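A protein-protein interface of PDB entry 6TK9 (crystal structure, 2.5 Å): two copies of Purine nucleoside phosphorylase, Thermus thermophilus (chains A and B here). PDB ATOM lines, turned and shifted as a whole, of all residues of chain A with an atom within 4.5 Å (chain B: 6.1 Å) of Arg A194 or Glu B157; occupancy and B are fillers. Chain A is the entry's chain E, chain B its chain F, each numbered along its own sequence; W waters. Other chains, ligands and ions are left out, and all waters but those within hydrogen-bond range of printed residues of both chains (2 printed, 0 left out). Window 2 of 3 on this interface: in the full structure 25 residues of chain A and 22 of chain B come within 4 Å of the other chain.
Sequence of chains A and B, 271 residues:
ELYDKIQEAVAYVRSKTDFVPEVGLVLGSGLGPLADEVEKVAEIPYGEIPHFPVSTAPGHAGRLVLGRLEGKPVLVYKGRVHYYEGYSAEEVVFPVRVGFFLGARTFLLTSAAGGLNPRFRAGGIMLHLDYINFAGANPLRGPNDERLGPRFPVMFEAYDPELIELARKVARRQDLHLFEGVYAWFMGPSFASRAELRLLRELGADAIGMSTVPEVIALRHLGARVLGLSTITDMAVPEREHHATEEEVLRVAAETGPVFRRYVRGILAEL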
ATOM      1  N   ALA A 192     -30.003  -0.872  -4.599  1.00  0.00           N
ATOM      2  CA  ALA A 192     -28.651  -0.522  -4.124  1.00  0.00           C
ATOM      3  C   ALA A 192     -27.625  -0.886  -5.209  1.00  0.00           C
ATOM      4  O   ALA A 192     -27.864  -1.840  -5.990  1.00  0.00           O
ATOM      5  CB  ALA A 192     -28.406  -1.226  -2.810  1.00  0.00           C
ATOM      6  N   SER A 193     -26.553  -0.099  -5.307  1.00  0.00           N
ATOM      7  CA  SER A 193     -25.311  -0.446  -6.038  1.00  0.00           C
ATOM      8  C   SER A 193     -24.672  -1.668  -5.388  1.00  0.00           C
ATOM      9  O   SER A 193     -24.929  -1.909  -4.190  1.00  0.00           O
ATOM     10  CB  SER A 193     -24.323   0.689  -6.022  1.00  0.00           C
ATOM     11  OG  SER A 193     -23.878   0.956  -4.688  1.00  0.00           O
ATOM     12  N   ARG A 194     -23.792  -2.330  -6.132  1.00  0.00           N
ATOM     13  CA  ARG A 194     -22.891  -3.391  -5.627  1.00  0.00           C
ATOM     14  C   ARG A 194     -22.186  -2.898  -4.349  1.00  0.00           C
ATOM     15  O   ARG A 194     -22.247  -3.607  -3.332  1.00  0.00           O
ATOM     16  CB  ARG A 194     -21.920  -3.815  -6.734  1.00  0.00           C
ATOM     17  CG  ARG A 194     -22.534  -4.723  -7.790  1.00  0.00           C
ATOM     18  CD  ARG A 194     -21.478  -5.240  -8.756  1.00  0.00           C
ATOM     19  NE  ARG A 194     -22.088  -5.723  -9.994  1.00  0.00           N
ATOM     20  CZ  ARG A 194     -22.625  -6.922 -10.175  1.00  0.00           C
ATOM     21  NH1 ARG A 194     -22.609  -7.838  -9.224  1.00  0.00           N
ATOM     22  NH2 ARG A 194     -23.181  -7.212 -11.323  1.00  0.00           N
ATOM     23  N   ALA A 195     -21.573  -1.715  -4.368  1.00  0.00           N
ATOM     24  CA  ALA A 195     -20.800  -1.170  -3.223  1.00  0.00           C
ATOM     25  C   ALA A 195     -21.719  -0.853  -2.024  1.00  0.00           C
ATOM     26  O   ALA A 195     -21.263  -0.968  -0.865  1.00  0.00           O
ATOM     27  CB  ALA A 195     -20.021   0.044  -3.674  1.00  0.00           C
ATOM     28  N   GLU A 196     -22.967  -0.440  -2.264  1.00  0.00           N
ATOM     29  CA  GLU A 196     -23.936  -0.118  -1.177  1.00  0.00           C
ATOM     30  C   GLU A 196     -24.351  -1.432  -0.506  1.00  0.00           C
ATOM     31  O   GLU A 196     -24.406  -1.455   0.715  1.00  0.00           O
ATOM     32  CB  GLU A 196     -25.132   0.677  -1.711  1.00  0.00           C
ATOM     33  CG  GLU A 196     -24.847   2.163  -1.940  1.00  0.00           C
ATOM     34  CD  GLU A 196     -25.929   2.942  -2.686  1.00  0.00           C
ATOM     35  OE1 GLU A 196     -26.761   2.313  -3.376  1.00  0.00           O
ATOM     36  OE2 GLU A 196     -25.954   4.187  -2.554  1.00  0.00           O
ATOM     37  N   LEU A 197     -24.576  -2.500  -1.271  1.00  0.00           N
ATOM     38  CA  LEU A 197     -24.858  -3.837  -0.704  1.00  0.00           C
ATOM     39  C   LEU A 197     -23.659  -4.274   0.140  1.00  0.00           C
ATOM     40  O   LEU A 197     -23.875  -4.728   1.250  1.00  0.00           O
ATOM     41  CB  LEU A 197     -25.132  -4.850  -1.820  1.00  0.00           C
ATOM     42  CG  LEU A 197     -26.429  -4.654  -2.603  1.00  0.00           C
ATOM     43  CD1 LEU A 197     -26.583  -5.764  -3.637  1.00  0.00           C
ATOM     44  CD2 LEU A 197     -27.631  -4.593  -1.674  1.00  0.00           C
ATOM     45  N   ARG A 198     -22.443  -4.188  -0.387  1.00  0.00           N
ATOM     46  CA  ARG A 198     -21.229  -4.639   0.339  1.00  0.00           C
ATOM     47  C   ARG A 198     -21.169  -3.867   1.663  1.00  0.00           C
ATOM     48  O   ARG A 198     -20.950  -4.490   2.711  1.00  0.00           O
ATOM     49  CB  ARG A 198     -19.972  -4.418  -0.508  1.00  0.00           C
ATOM     50  CG  ARG A 198     -18.682  -4.921   0.121  1.00  0.00           C
ATOM     51  CD  ARG A 198     -17.486  -4.349  -0.615  1.00  0.00           C
ATOM     52  NE  ARG A 198     -16.210  -4.579   0.056  1.00  0.00           N
ATOM     53  CZ  ARG A 198     -15.084  -3.887  -0.167  1.00  0.00           C
ATOM     54  NH1 ARG A 198     -15.059  -2.893  -1.043  1.00  0.00           N
ATOM     55  NH2 ARG A 198     -13.982  -4.190   0.501  1.00  0.00           N
ATOM     56  N   PRO A 238     -23.418  -8.647  -3.942  1.00  0.00           N
ATOM     57  CA  PRO A 238     -22.692  -7.856  -4.932  1.00  0.00           C
ATOM     58  C   PRO A 238     -21.621  -8.594  -5.746  1.00  0.00           C
ATOM     59  O   PRO A 238     -21.242  -8.050  -6.760  1.00  0.00           O
ATOM     60  CB  PRO A 238     -21.967  -6.757  -4.129  1.00  0.00           C
ATOM     61  CG  PRO A 238     -22.038  -7.193  -2.671  1.00  0.00           C
ATOM     62  CD  PRO A 238     -23.218  -8.142  -2.571  1.00  0.00           C
ATOM     63  N   ARG A 240     -22.019 -11.777  -6.777  1.00  0.00           N
ATOM     64  CA  ARG A 240     -22.816 -12.584  -7.748  1.00  0.00           C
ATOM     65  C   ARG A 240     -23.239 -11.643  -8.902  1.00  0.00           C
ATOM     66  O   ARG A 240     -23.282 -10.419  -8.658  1.00  0.00           O
ATOM     67  CB  ARG A 240     -23.983 -13.251  -7.008  1.00  0.00           C
ATOM     68  CG  ARG A 240     -23.802 -14.741  -6.723  1.00  0.00           C
ATOM     69  CD  ARG A 240     -23.600 -15.184  -5.278  1.00  0.00           C
ATOM     70  NE  ARG A 240     -24.868 -15.523  -4.673  1.00  0.00           N
ATOM     71  CZ  ARG A 240     -25.083 -16.249  -3.567  1.00  0.00           C
ATOM     72  NH1 ARG A 240     -24.103 -16.759  -2.837  1.00  0.00           N
ATOM     73  NH2 ARG A 240     -26.333 -16.447  -3.183  1.00  0.00           N
ATOM     74  N   GLU A 241     -23.505 -12.150 -10.113  1.00  0.00           N
ATOM     75  CA  GLU A 241     -24.059 -11.324 -11.221  1.00  0.00           C
ATOM     76  C   GLU A 241     -25.569 -11.193 -10.989  1.00  0.00           C
ATOM     77  O   GLU A 241     -26.170 -12.075 -10.333  1.00  0.00           O
ATOM     78  CB  GLU A 241     -23.662 -11.886 -12.599  1.00  0.00           C
ATOM     79  CG  GLU A 241     -24.724 -12.703 -13.341  1.00  0.00           C
ATOM     80  CD  GLU A 241     -25.507 -11.961 -14.432  1.00  0.00           C
ATOM     81  OE1 GLU A 241     -24.886 -11.119 -15.134  1.00  0.00           O
ATOM     82  OE2 GLU A 241     -26.740 -12.230 -14.596  1.00  0.00           O
ATOM     83  N   HIS A 242     -26.155 -10.120 -11.496  1.00  0.00           N
ATOM     84  CA  HIS A 242     -27.629  -9.920 -11.587  1.00  0.00           C
ATOM     85  C   HIS A 242     -28.267  -9.766 -10.208  1.00  0.00           C
ATOM     86  O   HIS A 242     -28.103 -10.629  -9.349  1.00  0.00           O
ATOM     87  CB  HIS A 242     -28.343 -10.965 -12.467  1.00  0.00           C
ATOM     88  CG  HIS A 242     -28.801 -10.381 -13.776  1.00  0.00           C
ATOM     89  ND1 HIS A 242     -30.121 -10.450 -14.211  1.00  0.00           N
ATOM     90  CD2 HIS A 242     -28.143  -9.655 -14.717  1.00  0.00           C
ATOM     91  CE1 HIS A 242     -30.239  -9.829 -15.373  1.00  0.00           C
ATOM     92  NE2 HIS A 242     -29.038  -9.328 -15.703  1.00  0.00           N
ATOM     93  N   ASP B 130     -18.263   2.235  -9.767  1.00  0.00           N
ATOM     94  CA  ASP B 130     -19.474   2.123  -8.906  1.00  0.00           C
ATOM     95  C   ASP B 130     -19.548   3.348  -7.993  1.00  0.00           C
ATOM     96  O   ASP B 130     -18.635   4.172  -8.032  1.00  0.00           O
ATOM     97  CB  ASP B 130     -19.495   0.804  -8.113  1.00  0.00           C
ATOM     98  CG  ASP B 130     -20.872   0.160  -7.981  1.00  0.00           C
ATOM     99  OD1 ASP B 130     -21.803   0.630  -8.651  1.00  0.00           O
ATOM    100  OD2 ASP B 130     -21.012  -0.804  -7.190  1.00  0.00           O
ATOM    101  N   TYR B 131     -20.632   3.480  -7.238  1.00  0.00           N
ATOM    102  CA  TYR B 131     -20.896   4.646  -6.373  1.00  0.00           C
ATOM    103  C   TYR B 131     -21.495   4.179  -5.047  1.00  0.00           C
ATOM    104  O   TYR B 131     -22.004   3.047  -4.946  1.00  0.00           O
ATOM    105  CB  TYR B 131     -21.881   5.603  -7.043  1.00  0.00           C
ATOM    106  CG  TYR B 131     -23.284   5.066  -7.134  1.00  0.00           C
ATOM    107  CD1 TYR B 131     -24.168   5.200  -6.077  1.00  0.00           C
ATOM    108  CD2 TYR B 131     -23.739   4.448  -8.288  1.00  0.00           C
ATOM    109  CE1 TYR B 131     -25.463   4.709  -6.154  1.00  0.00           C
ATOM    110  CE2 TYR B 131     -25.028   3.943  -8.379  1.00  0.00           C
ATOM    111  CZ  TYR B 131     -25.892   4.077  -7.310  1.00  0.00           C
ATOM    112  OH  TYR B 131     -27.150   3.563  -7.383  1.00  0.00           O
ATOM    113  N   MET B 155     -29.541  -1.085 -10.167  1.00  0.00           N
ATOM    114  CA  MET B 155     -28.366  -0.166 -10.167  1.00  0.00           C
ATOM    115  C   MET B 155     -27.059  -0.958 -10.286  1.00  0.00           C
ATOM    116  O   MET B 155     -25.985  -0.350 -10.187  1.00  0.00           O
ATOM    117  CB  MET B 155     -28.332   0.688  -8.898  1.00  0.00           C
ATOM    118  CG  MET B 155     -29.450   1.725  -8.861  1.00  0.00           C
ATOM    119  SD  MET B 155     -29.575   2.670 -10.414  1.00  0.00           S
ATOM    120  CE  MET B 155     -28.037   3.578 -10.317  1.00  0.00           C
ATOM    121  N   PHE B 156     -27.151  -2.262 -10.526  1.00  0.00           N
ATOM    122  CA  PHE B 156     -26.015  -3.097 -10.991  1.00  0.00           C
ATOM    123  C   PHE B 156     -25.624  -2.573 -12.372  1.00  0.00           C
ATOM    124  O   PHE B 156     -26.528  -2.243 -13.150  1.00  0.00           O
ATOM    125  CB  PHE B 156     -26.376  -4.594 -10.984  1.00  0.00           C
ATOM    126  CG  PHE B 156     -26.264  -5.304  -9.649  1.00  0.00           C
ATOM    127  CD1 PHE B 156     -26.488  -4.636  -8.443  1.00  0.00           C
ATOM    128  CD2 PHE B 156     -25.958  -6.660  -9.603  1.00  0.00           C
ATOM    129  CE1 PHE B 156     -26.372  -5.298  -7.226  1.00  0.00           C
ATOM    130  CE2 PHE B 156     -25.826  -7.321  -8.386  1.00  0.00           C
ATOM    131  CZ  PHE B 156     -26.038  -6.635  -7.198  1.00  0.00           C
ATOM    132  N   GLU B 157     -24.327  -2.437 -12.656  1.00  0.00           N
ATOM    133  CA  GLU B 157     -23.837  -2.020 -13.996  1.00  0.00           C
ATOM    134  C   GLU B 157     -24.328  -0.597 -14.273  1.00  0.00           C
ATOM    135  O   GLU B 157     -24.559  -0.256 -15.433  1.00  0.00           O
ATOM    136  CB  GLU B 157     -24.289  -3.036 -15.052  1.00  0.00           C
ATOM    137  CG  GLU B 157     -23.242  -4.084 -15.357  1.00  0.00           C
ATOM    138  CD  GLU B 157     -22.946  -5.032 -14.217  1.00  0.00           C
ATOM    139  OE1 GLU B 157     -23.814  -5.881 -13.934  1.00  0.00           O
ATOM    140  OE2 GLU B 157     -21.856  -4.911 -13.609  1.00  0.00           O
ATOM    141  N   ALA B 158     -24.480   0.206 -13.223  1.00  0.00           N
ATOM    142  CA  ALA B 158     -24.861   1.633 -13.316  1.00  0.00           C
ATOM    143  C   ALA B 158     -23.901   2.309 -14.299  1.00  0.00           C
ATOM    144  O   ALA B 158     -24.353   2.817 -15.342  1.00  0.00           O
ATOM    145  CB  ALA B 158     -24.810   2.270 -11.950  1.00  0.00           C
ATOM    146  N   TYR B 159     -22.614   2.274 -13.985  1.00  0.00           N
ATOM    147  CA  TYR B 159     -21.549   2.671 -14.934  1.00  0.00           C
ATOM    148  C   TYR B 159     -21.463   1.545 -15.954  1.00  0.00           C
ATOM    149  O   TYR B 159     -21.177   0.457 -15.535  1.00  0.00           O
ATOM    150  CB  TYR B 159     -20.243   3.001 -14.202  1.00  0.00           C
ATOM    151  CG  TYR B 159     -20.361   4.139 -13.210  1.00  0.00           C
ATOM    152  CD1 TYR B 159     -20.458   5.459 -13.615  1.00  0.00           C
ATOM    153  CD2 TYR B 159     -20.381   3.902 -11.857  1.00  0.00           C
ATOM    154  CE1 TYR B 159     -20.589   6.501 -12.707  1.00  0.00           C
ATOM    155  CE2 TYR B 159     -20.503   4.932 -10.938  1.00  0.00           C
ATOM    156  CZ  TYR B 159     -20.607   6.243 -11.354  1.00  0.00           C
ATOM    157  OH  TYR B 159     -20.707   7.246 -10.410  1.00  0.00           O
ATOM    158  N   ASP B 160     -21.804   1.818 -17.216  1.00  0.00           N
ATOM    159  CA  ASP B 160     -21.804   0.849 -18.347  1.00  0.00           C
ATOM    160  C   ASP B 160     -20.483   0.079 -18.404  1.00  0.00           C
ATOM    161  O   ASP B 160     -19.423   0.693 -18.382  1.00  0.00           O
ATOM    162  CB  ASP B 160     -22.032   1.564 -19.683  1.00  0.00           C
ATOM    163  CG  ASP B 160     -22.356   0.600 -20.806  1.00  0.00           C
ATOM    164  OD1 ASP B 160     -23.534   0.180 -20.899  1.00  0.00           O
ATOM    165  OD2 ASP B 160     -21.417   0.227 -21.531  1.00  0.00           O
ATOM    166  N   PRO B 161     -20.496  -1.273 -18.474  1.00  0.00           N
ATOM    167  CA  PRO B 161     -19.290  -2.074 -18.706  1.00  0.00           C
ATOM    168  C   PRO B 161     -18.549  -1.932 -20.043  1.00  0.00           C
ATOM    169  O   PRO B 161     -17.360  -2.127 -20.031  1.00  0.00           O
ATOM    170  CB  PRO B 161     -19.774  -3.533 -18.706  1.00  0.00           C
ATOM    171  CG  PRO B 161     -21.083  -3.501 -17.973  1.00  0.00           C
ATOM    172  CD  PRO B 161     -21.666  -2.125 -18.227  1.00  0.00           C
ATOM    173  N   ARG B 220     -29.989   6.024 -15.122  1.00  0.00           N
ATOM    174  CA  ARG B 220     -30.243   4.556 -15.165  1.00  0.00           C
ATOM    175  C   ARG B 220     -31.755   4.306 -15.101  1.00  0.00           C
ATOM    176  O   ARG B 220     -32.236   3.434 -15.835  1.00  0.00           O
ATOM    177  CB  ARG B 220     -29.482   3.804 -14.066  1.00  0.00           C
ATOM    178  CG  ARG B 220     -27.967   3.851 -14.220  1.00  0.00           C
ATOM    179  CD  ARG B 220     -27.530   3.346 -15.573  1.00  0.00           C
ATOM    180  NE  ARG B 220     -27.856   1.942 -15.722  1.00  0.00           N
ATOM    181  CZ  ARG B 220     -28.181   1.342 -16.852  1.00  0.00           C
ATOM    182  NH1 ARG B 220     -28.281   2.031 -17.976  1.00  0.00           N
ATOM    183  NH2 ARG B 220     -28.466   0.055 -16.837  1.00  0.00           N
HETATM  184  O   HOH W   1     -29.322  -3.073  -7.850  1.00  0.00           O
HETATM  185  O   HOH W   2     -28.655   3.070  -5.293  1.00  0.00           O
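Of the printed residues of chain B, Ser A193 touches Asp B130 and Tyr B131. Of chain B, only Asp B130 (3.2 Å), Phe B156 (3.3 Å) and Glu B157 (3.0 Å) come within 4 Å of Arg A194. Of the printed residues of chain B, Ala A195 touches Asp B130 and Tyr B131. Printed residues of chain B within 4 Å of His A242: Phe B156 (3.9 Å). Printed residues of chain A within 4 Å of Asp B130: Ser A193, Arg A194 and Ala A195. Printed residues of chain A within 4 Å of Phe B156: Ala A192 (3.96 Å), Arg A194 (3.3 Å), Leu A197 (3.6 Å) and His A242 (3.9 Å). Glu B157 touches just one residue of chain A: Arg A194. Ala B158 touches none of the printed residues of chain A. The nearest residue of chain B that does not touch Arg A194 is Met B155 (5.0 Å). The nearest printed residue of chain A that does not touch Glu B157 is His A242 (5.4 Å).
No position is printed for both chains. Of the 12 pairs that touch across the chains among the printed residues, none has its exchanged pair printed and touching as well.
Among the printed residues, pairs that only touch across the chains: Arg A194 with Phe B156, Leu A197 with Phe B156, Ser A193 with Asp B130, Glu A196 with Tyr B131, Ala A195 with Tyr B131, Ala A192 with Met B155, His A242 with Phe B156 and Ala A192 with Phe B156.
Hydrophobic or aromatic side chains of chain A within 4 Å of the printed part of chain B: Ala A195 and Leu A197. Of the 10 printed residues of chain B, 5 touch a printed residue of chain A. Printed residues of chain B that touch a printed residue of chain A: Asp B130, Tyr B131, Met B155, Phe B156 and Glu B157. Among the printed residues, Asp or Glu carboxylates within 4 Å of a Lys or Arg side-chain nitrogen of the other chain: Arg A194 with Glu B157 (3.0 Å).
The side-chain hydroxyl (OG) of Ser A193 sits at hydrogen-bond distance from the backbone NH (N) of Glu A196, 2.9 Å away. The backbone carbonyl oxygen (O) of Arg A240 sits at hydrogen-bond distance from the guanidinium group (NH1) of Arg A194 (2.7 Å). The backbone carbonyl oxygen (O) of Pro A238 lies within hydrogen-bond range of the guanidinium group (NH1) of Arg A194, at 2.8 Å.
Water W2 lies within hydrogen-bond range of the side-chain hydroxyl of Tyr B131 (2.6 Å) and the side-chain carboxylate of Glu A196 (2.8 Å). Water W1 lies within hydrogen-bond range of O of Ala A192 (2.7 Å) and N of Met B155 (3.1 Å).
The side-chain hydroxyl (OG) of Ser A193 is in hydrogen-bond range of the backbone carbonyl oxygen (O) of Tyr B131 (2.8 Å). The backbone NH (N) of Ala A195 sits at hydrogen-bond distance from the side-chain carboxylate (OD2) of Asp B130. NH2 of Arg A194 is in salt-bridge range of OE1 of Glu B157, at 3.0 Å. N of Arg A194 sits close to OD2 of Asp B130, at 3.3 Å.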
